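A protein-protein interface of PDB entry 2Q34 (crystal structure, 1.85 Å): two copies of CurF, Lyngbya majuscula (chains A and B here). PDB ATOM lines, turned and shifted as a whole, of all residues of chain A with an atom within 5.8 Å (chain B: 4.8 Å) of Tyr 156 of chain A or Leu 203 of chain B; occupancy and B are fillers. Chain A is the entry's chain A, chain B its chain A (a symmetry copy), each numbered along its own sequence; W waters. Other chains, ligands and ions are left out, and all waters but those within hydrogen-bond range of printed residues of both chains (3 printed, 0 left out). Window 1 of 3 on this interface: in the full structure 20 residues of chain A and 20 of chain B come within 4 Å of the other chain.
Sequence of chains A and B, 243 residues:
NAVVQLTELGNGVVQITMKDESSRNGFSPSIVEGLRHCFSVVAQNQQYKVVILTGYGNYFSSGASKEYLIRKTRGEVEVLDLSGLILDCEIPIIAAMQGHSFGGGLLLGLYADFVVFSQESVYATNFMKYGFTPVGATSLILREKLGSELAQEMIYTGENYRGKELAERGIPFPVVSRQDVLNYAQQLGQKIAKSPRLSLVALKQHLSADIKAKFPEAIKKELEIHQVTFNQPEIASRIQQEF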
ATOM      1  N   THR A 125     -12.328  28.964  15.436  1.00  0.00           N
ATOM      2  CA  THR A 125     -13.607  29.428  15.918  1.00  0.00           C
ATOM      3  C   THR A 125     -13.282  29.625  17.387  1.00  0.00           C
ATOM      4  O   THR A 125     -13.342  28.673  18.169  1.00  0.00           O
ATOM      5  CB  THR A 125     -14.707  28.346  15.774  1.00  0.00           C
ATOM      6  OG1 THR A 125     -14.310  27.162  16.472  1.00  0.00           O
ATOM      7  CG2 THR A 125     -14.886  27.963  14.332  1.00  0.00           C
ATOM      8  N   MET A 128     -14.932  30.232  22.298  1.00  0.00           N
ATOM      9  CA  MET A 128     -14.683  29.567  23.574  1.00  0.00           C
ATOM     10  C   MET A 128     -13.354  29.947  24.221  1.00  0.00           C
ATOM     11  O   MET A 128     -13.194  29.805  25.429  1.00  0.00           O
ATOM     12  CB  MET A 128     -14.854  28.055  23.456  1.00  0.00           C
ATOM     13  CG  MET A 128     -16.324  27.669  23.275  1.00  0.00           C
ATOM     14  SD  MET A 128     -17.383  27.897  24.886  1.00  0.00           S
ATOM     15  CE  MET A 128     -16.917  26.175  25.757  1.00  0.00           C
ATOM     16  N   THR A 133     -20.041  30.929  24.130  1.00  0.00           N
ATOM     17  CA  THR A 133     -20.459  30.066  23.034  1.00  0.00           C
ATOM     18  C   THR A 133     -20.577  30.862  21.721  1.00  0.00           C
ATOM     19  O   THR A 133     -20.697  32.093  21.750  1.00  0.00           O
ATOM     20  CB  THR A 133     -21.773  29.321  23.386  1.00  0.00           C
ATOM     21  OG1 THR A 133     -22.800  30.268  23.711  1.00  0.00           O
ATOM     22  CG2 THR A 133     -21.558  28.379  24.582  1.00  0.00           C
ATOM     23  N   PRO A 134     -20.519  30.161  20.578  1.00  0.00           N
ATOM     24  CA  PRO A 134     -20.522  30.781  19.256  1.00  0.00           C
ATOM     25  C   PRO A 134     -21.826  31.468  18.830  1.00  0.00           C
ATOM     26  O   PRO A 134     -22.896  31.232  19.402  1.00  0.00           O
ATOM     27  CB  PRO A 134     -20.263  29.591  18.309  1.00  0.00           C
ATOM     28  CG  PRO A 134     -19.664  28.538  19.171  1.00  0.00           C
ATOM     29  CD  PRO A 134     -20.380  28.692  20.477  1.00  0.00           C
ATOM     30  N   ALA A 151     -15.173  19.716  13.814  1.00  0.00           N
ATOM     31  CA  ALA A 151     -15.976  20.857  14.227  1.00  0.00           C
ATOM     32  C   ALA A 151     -16.010  20.918  15.755  1.00  0.00           C
ATOM     33  O   ALA A 151     -15.772  21.965  16.349  1.00  0.00           O
ATOM     34  CB  ALA A 151     -17.390  20.766  13.647  1.00  0.00           C
ATOM     35  N   GLN A 152     -16.262  19.778  16.389  1.00  0.00           N
ATOM     36  CA  GLN A 152     -16.394  19.760  17.844  1.00  0.00           C
ATOM     37  C   GLN A 152     -15.111  20.177  18.578  1.00  0.00           C
ATOM     38  O   GLN A 152     -15.162  20.979  19.510  1.00  0.00           O
ATOM     39  CB  GLN A 152     -16.864  18.392  18.304  1.00  0.00           C
ATOM     40  CG  GLN A 152     -17.669  18.460  19.559  1.00  0.00           C
ATOM     41  CD  GLN A 152     -18.730  17.397  19.604  1.00  0.00           C
ATOM     42  OE1 GLN A 152     -19.644  17.380  18.780  1.00  0.00           O
ATOM     43  NE2 GLN A 152     -18.614  16.502  20.556  1.00  0.00           N
ATOM     44  N   GLU A 153     -13.968  19.657  18.147  1.00  0.00           N
ATOM     45  CA  GLU A 153     -12.705  20.044  18.748  1.00  0.00           C
ATOM     46  C   GLU A 153     -12.447  21.528  18.588  1.00  0.00           C
ATOM     47  O   GLU A 153     -12.139  22.212  19.552  1.00  0.00           O
ATOM     48  CB  GLU A 153     -11.539  19.272  18.156  1.00  0.00           C
ATOM     49  CG  GLU A 153     -10.283  19.453  18.994  1.00  0.00           C
ATOM     50  CD  GLU A 153      -9.107  18.779  18.369  1.00  0.00           C
ATOM     51  OE1 GLU A 153      -9.142  17.543  18.264  1.00  0.00           O
ATOM     52  OE2 GLU A 153      -8.161  19.486  17.974  1.00  0.00           O
ATOM     53  N   MET A 154     -12.578  22.025  17.364  1.00  0.00           N
ATOM     54  CA  MET A 154     -12.394  23.451  17.118  1.00  0.00           C
ATOM     55  C   MET A 154     -13.309  24.325  17.962  1.00  0.00           C
ATOM     56  O   MET A 154     -12.851  25.311  18.540  1.00  0.00           O
ATOM     57  CB  MET A 154     -12.579  23.755  15.630  1.00  0.00           C
ATOM     58  CG  MET A 154     -11.547  23.055  14.793  1.00  0.00           C
ATOM     59  SD  MET A 154     -11.635  23.747  12.951  1.00  0.00           S
ATOM     60  CE  MET A 154     -10.914  25.546  13.274  1.00  0.00           C
ATOM     61  N   ILE A 155     -14.575  23.948  18.084  1.00  0.00           N
ATOM     62  CA  ILE A 155     -15.517  24.781  18.847  1.00  0.00           C
ATOM     63  C   ILE A 155     -15.253  24.720  20.352  1.00  0.00           C
ATOM     64  O   ILE A 155     -15.267  25.746  21.029  1.00  0.00           O
ATOM     65  CB  ILE A 155     -16.984  24.443  18.564  1.00  0.00           C
ATOM     66  CG1 ILE A 155     -17.315  24.704  17.085  1.00  0.00           C
ATOM     67  CG2 ILE A 155     -17.905  25.330  19.432  1.00  0.00           C
ATOM     68  CD1 ILE A 155     -18.603  24.042  16.643  1.00  0.00           C
ATOM     69  N   TYR A 156     -15.009  23.526  20.885  1.00  0.00           N
ATOM     70  CA  TYR A 156     -14.804  23.416  22.336  1.00  0.00           C
ATOM     71  C   TYR A 156     -13.518  24.063  22.821  1.00  0.00           C
ATOM     72  O   TYR A 156     -13.511  24.702  23.886  1.00  0.00           O
ATOM     73  CB  TYR A 156     -14.738  21.956  22.774  1.00  0.00           C
ATOM     74  CG  TYR A 156     -16.032  21.316  23.190  1.00  0.00           C
ATOM     75  CD1 TYR A 156     -16.512  21.443  24.502  1.00  0.00           C
ATOM     76  CD2 TYR A 156     -16.741  20.515  22.304  1.00  0.00           C
ATOM     77  CE1 TYR A 156     -17.681  20.814  24.901  1.00  0.00           C
ATOM     78  CE2 TYR A 156     -17.902  19.871  22.703  1.00  0.00           C
ATOM     79  CZ  TYR A 156     -18.374  20.032  24.000  1.00  0.00           C
ATOM     80  OH  TYR A 156     -19.516  19.369  24.389  1.00  0.00           O
ATOM     81  N   THR A 157     -12.432  23.867  22.074  1.00  0.00           N
ATOM     82  CA  THR A 157     -11.119  24.409  22.461  1.00  0.00           C
ATOM     83  C   THR A 157     -10.948  25.899  22.121  1.00  0.00           C
ATOM     84  O   THR A 157     -10.254  26.622  22.839  1.00  0.00           O
ATOM     85  CB  THR A 157      -9.921  23.616  21.867  1.00  0.00           C
ATOM     86  OG1 THR A 157      -9.788  23.888  20.468  1.00  0.00           O
ATOM     87  CG2 THR A 157     -10.047  22.130  22.090  1.00  0.00           C
ATOM     88  N   GLY A 158     -11.561  26.336  21.029  1.00  0.00           N
ATOM     89  CA  GLY A 158     -11.361  27.681  20.497  1.00  0.00           C
ATOM     90  C   GLY A 158      -9.947  27.947  19.983  1.00  0.00           C
ATOM     91  O   GLY A 158      -9.602  29.093  19.682  1.00  0.00           O
ATOM     92  N   ILE A 225     -28.204  31.140  23.514  1.00  0.00           N
ATOM     93  CA  ILE A 225     -27.187  30.528  24.384  1.00  0.00           C
ATOM     94  C   ILE A 225     -26.002  31.486  24.562  1.00  0.00           C
ATOM     95  O   ILE A 225     -25.465  31.649  25.667  1.00  0.00           O
ATOM     96  CB  ILE A 225     -26.741  29.153  23.821  1.00  0.00           C
ATOM     97  CG1 ILE A 225     -27.948  28.214  23.710  1.00  0.00           C
ATOM     98  CG2 ILE A 225     -25.604  28.532  24.677  1.00  0.00           C
ATOM     99  CD1 ILE A 225     -27.702  27.000  22.827  1.00  0.00           C
ATOM    100  N   PRO B  92     -18.451  17.468  29.175  1.00  0.00           N
ATOM    101  CA  PRO B  92     -17.790  16.687  28.125  1.00  0.00           C
ATOM    102  C   PRO B  92     -17.013  15.483  28.657  1.00  0.00           C
ATOM    103  O   PRO B  92     -16.343  15.575  29.709  1.00  0.00           O
ATOM    104  CB  PRO B  92     -16.774  17.669  27.507  1.00  0.00           C
ATOM    105  CG  PRO B  92     -17.073  18.993  28.088  1.00  0.00           C
ATOM    106  CD  PRO B  92     -18.049  18.891  29.182  1.00  0.00           C
ATOM    107  N   ASP B 113     -18.124  12.449  23.963  1.00  0.00           N
ATOM    108  CA  ASP B 113     -17.987  13.605  23.087  1.00  0.00           C
ATOM    109  C   ASP B 113     -16.722  13.531  22.234  1.00  0.00           C
ATOM    110  O   ASP B 113     -16.736  13.957  21.066  1.00  0.00           O
ATOM    111  CB  ASP B 113     -18.047  14.869  23.934  1.00  0.00           C
ATOM    112  CG  ASP B 113     -19.296  14.891  24.806  1.00  0.00           C
ATOM    113  OD1 ASP B 113     -20.400  15.136  24.275  1.00  0.00           O
ATOM    114  OD2 ASP B 113     -19.194  14.581  26.002  1.00  0.00           O
ATOM    115  N   PHE B 114     -15.649  12.979  22.797  1.00  0.00           N
ATOM    116  CA  PHE B 114     -14.391  12.810  22.066  1.00  0.00           C
ATOM    117  C   PHE B 114     -13.911  11.383  22.314  1.00  0.00           C
ATOM    118  O   PHE B 114     -14.213  10.798  23.349  1.00  0.00           O
ATOM    119  CB  PHE B 114     -13.324  13.782  22.586  1.00  0.00           C
ATOM    120  CG  PHE B 114     -13.722  15.229  22.427  1.00  0.00           C
ATOM    121  CD1 PHE B 114     -14.471  15.866  23.411  1.00  0.00           C
ATOM    122  CD2 PHE B 114     -13.377  15.926  21.278  1.00  0.00           C
ATOM    123  CE1 PHE B 114     -14.839  17.207  23.259  1.00  0.00           C
ATOM    124  CE2 PHE B 114     -13.748  17.259  21.131  1.00  0.00           C
ATOM    125  CZ  PHE B 114     -14.492  17.879  22.120  1.00  0.00           C
ATOM    126  N   ILE B 192      -9.785  21.702  26.886  1.00  0.00           N
ATOM    127  CA  ILE B 192     -11.223  21.947  27.022  1.00  0.00           C
ATOM    128  C   ILE B 192     -11.561  22.622  28.355  1.00  0.00           C
ATOM    129  O   ILE B 192     -12.363  23.572  28.396  1.00  0.00           O
ATOM    130  CB  ILE B 192     -12.010  20.622  26.840  1.00  0.00           C
ATOM    131  CG1 ILE B 192     -11.818  20.127  25.399  1.00  0.00           C
ATOM    132  CG2 ILE B 192     -13.503  20.808  27.148  1.00  0.00           C
ATOM    133  CD1 ILE B 192     -12.235  18.659  25.204  1.00  0.00           C
ATOM    134  N   SER B 195     -12.194  26.582  29.463  1.00  0.00           N
ATOM    135  CA  SER B 195     -13.465  27.309  29.403  1.00  0.00           C
ATOM    136  C   SER B 195     -14.229  27.251  30.713  1.00  0.00           C
ATOM    137  O   SER B 195     -14.058  26.296  31.495  1.00  0.00           O
ATOM    138  CB  SER B 195     -14.327  26.749  28.265  1.00  0.00           C
ATOM    139  OG  SER B 195     -13.681  27.014  27.033  1.00  0.00           O
ATOM    140  N   SER B 199     -20.255  27.491  30.287  1.00  0.00           N
ATOM    141  CA  SER B 199     -20.163  27.511  28.844  1.00  0.00           C
ATOM    142  C   SER B 199     -20.016  26.086  28.289  1.00  0.00           C
ATOM    143  O   SER B 199     -20.648  25.740  27.292  1.00  0.00           O
ATOM    144  CB  SER B 199     -19.004  28.400  28.408  1.00  0.00           C
ATOM    145  OG  SER B 199     -19.285  29.752  28.774  1.00  0.00           O
ATOM    146  N   LEU B 200     -19.185  25.272  28.936  1.00  0.00           N
ATOM    147  CA  LEU B 200     -19.027  23.870  28.521  1.00  0.00           C
ATOM    148  C   LEU B 200     -20.367  23.125  28.560  1.00  0.00           C
ATOM    149  O   LEU B 200     -20.704  22.370  27.630  1.00  0.00           O
ATOM    150  CB  LEU B 200     -17.974  23.154  29.393  1.00  0.00           C
ATOM    151  CG  LEU B 200     -16.508  23.574  29.234  1.00  0.00           C
ATOM    152  CD1 LEU B 200     -15.689  22.805  30.291  1.00  0.00           C
ATOM    153  CD2 LEU B 200     -16.046  23.211  27.797  1.00  0.00           C
ATOM    154  N   VAL B 201     -21.135  23.335  29.626  1.00  0.00           N
ATOM    155  CA  VAL B 201     -22.391  22.629  29.798  1.00  0.00           C
ATOM    156  C   VAL B 201     -23.407  23.079  28.723  1.00  0.00           C
ATOM    157  O   VAL B 201     -24.093  22.239  28.086  1.00  0.00           O
ATOM    158  CB  VAL B 201     -22.958  22.803  31.240  1.00  0.00           C
ATOM    159  CG1 VAL B 201     -24.385  22.266  31.323  1.00  0.00           C
ATOM    160  CG2 VAL B 201     -22.051  22.048  32.261  1.00  0.00           C
ATOM    161  N   ALA B 202     -23.475  24.390  28.507  1.00  0.00           N
ATOM    162  CA  ALA B 202     -24.396  24.977  27.526  1.00  0.00           C
ATOM    163  C   ALA B 202     -24.046  24.517  26.121  1.00  0.00           C
ATOM    164  O   ALA B 202     -24.930  24.206  25.301  1.00  0.00           O
ATOM    165  CB  ALA B 202     -24.326  26.509  27.581  1.00  0.00           C
ATOM    166  N   LEU B 203     -22.754  24.493  25.830  1.00  0.00           N
ATOM    167  CA  LEU B 203     -22.316  24.087  24.507  1.00  0.00           C
ATOM    168  C   LEU B 203     -22.624  22.608  24.281  1.00  0.00           C
ATOM    169  O   LEU B 203     -23.117  22.216  23.217  1.00  0.00           O
ATOM    170  CB  LEU B 203     -20.816  24.335  24.337  1.00  0.00           C
ATOM    171  CG  LEU B 203     -20.208  23.910  22.990  1.00  0.00           C
ATOM    172  CD1 LEU B 203     -20.838  24.669  21.855  1.00  0.00           C
ATOM    173  CD2 LEU B 203     -18.697  24.158  23.023  1.00  0.00           C
ATOM    174  N   LYS B 204     -22.314  21.782  25.269  1.00  0.00           N
ATOM    175  CA  LYS B 204     -22.553  20.339  25.124  1.00  0.00           C
ATOM    176  C   LYS B 204     -24.040  20.040  24.911  1.00  0.00           C
ATOM    177  O   LYS B 204     -24.394  19.219  24.066  1.00  0.00           O
ATOM    178  CB  LYS B 204     -22.010  19.563  26.334  1.00  0.00           C
ATOM    179  CG  LYS B 204     -22.431  18.083  26.286  1.00  0.00           C
ATOM    180  CD  LYS B 204     -21.628  17.235  27.237  1.00  0.00           C
ATOM    181  CE  LYS B 204     -22.260  15.834  27.302  1.00  0.00           C
ATOM    182  NZ  LYS B 204     -21.243  14.844  27.762  1.00  0.00           N
ATOM    183  N   GLN B 205     -24.916  20.740  25.635  1.00  0.00           N
ATOM    184  CA  GLN B 205     -26.341  20.542  25.486  1.00  0.00           C
ATOM    185  C   GLN B 205     -26.779  20.891  24.045  1.00  0.00           C
ATOM    186  O   GLN B 205     -27.539  20.154  23.413  1.00  0.00           O
ATOM    187  CB  GLN B 205     -27.102  21.401  26.485  1.00  0.00           C
ATOM    188  CG  GLN B 205     -28.613  21.190  26.408  1.00  0.00           C
ATOM    189  CD  GLN B 205     -29.340  21.876  27.518  1.00  0.00           C
ATOM    190  OE1 GLN B 205     -29.805  21.229  28.442  1.00  0.00           O
ATOM    191  NE2 GLN B 205     -29.442  23.194  27.444  1.00  0.00           N
ATOM    192  N   HIS B 206     -26.262  22.004  23.549  1.00  0.00           N
ATOM    193  CA  HIS B 206     -26.557  22.469  22.192  1.00  0.00           C
ATOM    194  C   HIS B 206     -26.103  21.433  21.151  1.00  0.00           C
ATOM    195  O   HIS B 206     -26.896  21.017  20.292  1.00  0.00           O
ATOM    196  CB  HIS B 206     -25.875  23.834  21.944  1.00  0.00           C
ATOM    197  CG  HIS B 206     -26.033  24.348  20.534  1.00  0.00           C
ATOM    198  ND1 HIS B 206     -27.251  24.717  20.011  1.00  0.00           N
ATOM    199  CD2 HIS B 206     -25.127  24.531  19.539  1.00  0.00           C
ATOM    200  CE1 HIS B 206     -27.095  25.104  18.755  1.00  0.00           C
ATOM    201  NE2 HIS B 206     -25.814  24.998  18.444  1.00  0.00           N
ATOM    202  N   LEU B 207     -24.833  21.039  21.222  1.00  0.00           N
ATOM    203  CA  LEU B 207     -24.236  20.138  20.232  1.00  0.00           C
ATOM    204  C   LEU B 207     -24.857  18.728  20.217  1.00  0.00           C
ATOM    205  O   LEU B 207     -24.927  18.084  19.153  1.00  0.00           O
ATOM    206  CB  LEU B 207     -22.718  20.019  20.444  1.00  0.00           C
ATOM    207  CG  LEU B 207     -21.842  21.257  20.144  1.00  0.00           C
ATOM    208  CD1 LEU B 207     -20.398  21.067  20.566  1.00  0.00           C
ATOM    209  CD2 LEU B 207     -21.908  21.586  18.665  1.00  0.00           C
HETATM  210  O   HOH W   1     -20.461  17.590  22.617  1.00  0.00           O
HETATM  211  O   HOH W   2     -11.199  28.430  26.793  1.00  0.00           O
HETATM  212  O   HOH W   3     -12.048  25.469  26.097  1.00  0.00           O
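No position is printed for both chains.
Among the printed residues, pairs that only touch across the chains: Met 128 of chain A with Ser 199 of chain B (3.9 Å), Met 128 of chain A with Leu 200 of chain B (3.7 Å), Met 128 of chain A with Leu 203 of chain B (3.8 Å), Thr 133 of chain A with Ser 199 of chain B (3.9 Å), Gln 152 of chain A with Leu 207 of chain B (3.9 Å), Glu 153 of chain A with Phe 114 of chain B (3.8 Å), Ile 155 of chain A with Leu 203 of chain B (3.9 Å), Tyr 156 of chain A with Pro 92 of chain B (3.7 Å), Tyr 156 of chain A with Phe 114 of chain B (3.5 Å), Tyr 156 of chain A with Ser 195 of chain B (3.9 Å), Tyr 156 of chain A with Leu 200 of chain B (3.8 Å), Tyr 156 of chain A with Leu 203 of chain B (3.8 Å), Tyr 156 of chain A with Lys 204 of chain B (3.2 Å), Tyr 156 of chain A with Leu 207 of chain B (3.5 Å), Ile 225 of chain A with Ala 202 of chain B (3.8 Å) and Ile 225 of chain A with His 206 of chain B (3.7 Å).
Of chain B, only Pro 92 (3.7 Å), Phe 114 (3.5 Å), Ser 195 (3.9 Å), Leu 200 (3.8 Å), Leu 203 (3.8 Å), Lys 204 (3.2 Å) and Leu 207 (3.5 Å) come within 4 Å of Tyr 156 of chain A.
Leu 203 of chain B touches three residues of chain A.
Of the printed residues of chain A, Asp 113 of chain B touches Gln 152 (3.2 Å).
Of the printed residues of chain A, Leu 207 of chain B touches Gln 152 (3.9 Å) and Tyr 156 (3.5 Å).
Of the printed residues of chain A, Lys 204 of chain B touches Tyr 156.
Thr 125 of chain A touches none of the printed residues of chain B.
Val 201 of chain B touches none of the printed residues of chain A.
The nearest residue of chain B that does not touch Tyr 156 of chain A is Ile 192 of chain B (4.1 Å).
The nearest residue of chain A that does not touch Leu 203 of chain B is Thr 133 of chain A (4.1 Å).
Of the 13 printed residues of chain A, 7 touch a printed residue of chain B.
Printed residues of chain A that touch a printed residue of chain B: Met 128, Thr 133, Gln 152, Glu 153, Ile 155, Tyr 156 and Ile 225.
Of the 14 printed residues of chain B, 11 touch a printed residue of chain A.
Hydrophobic or aromatic side chains of chain B that line the printed part of chain A: Pro 92, Phe 114, Leu 200, Ala 202, Leu 203, His 206 and Leu 207.
Among the printed residues, no Asp or Glu carboxylate lies within 4 Å of a Lys or Arg side-chain nitrogen of the other chain.
Water W3 lies within hydrogen-bond range of OG of Ser 195 of chain B, O of Tyr 156 of chain A and O of Ile 192 of chain B.
Water W1 lies within hydrogen-bond range of the side-chain hydroxyl of Tyr 156 of chain A (2.7 Å), the side-chain carboxylate of Asp 113 of chain B (3.0 Å) and the side-chain amide nitrogen of Gln 152 of chain A (3.0 Å).
Water W2 lies within hydrogen-bond range of the backbone carbonyl oxygen of Met 128 of chain A (2.8 Å) and the side-chain hydroxyl of Ser 195 of chain B (2.9 Å).
The backbone carbonyl oxygen of Glu 153 of chain A sits at hydrogen-bond distance from the side-chain hydroxyl of Thr 157 of chain A.
The side-chain carboxylate (OD2) of Asp 113 of chain B is in salt-bridge range of the side-chain amino group (NZ) of Lys 204 of chain B, 2.7 Å away.
The backbone carbonyl oxygen (O) of Met 128 of chain A lies within hydrogen-bond range of the side-chain hydroxyl (OG) of Ser 195 of chain B (3.3 Å).
The side-chain amide nitrogen of Gln 152 of chain A is in hydrogen-bond range of the backbone carbonyl oxygen of Asp 113 of chain B (3.2 Å).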
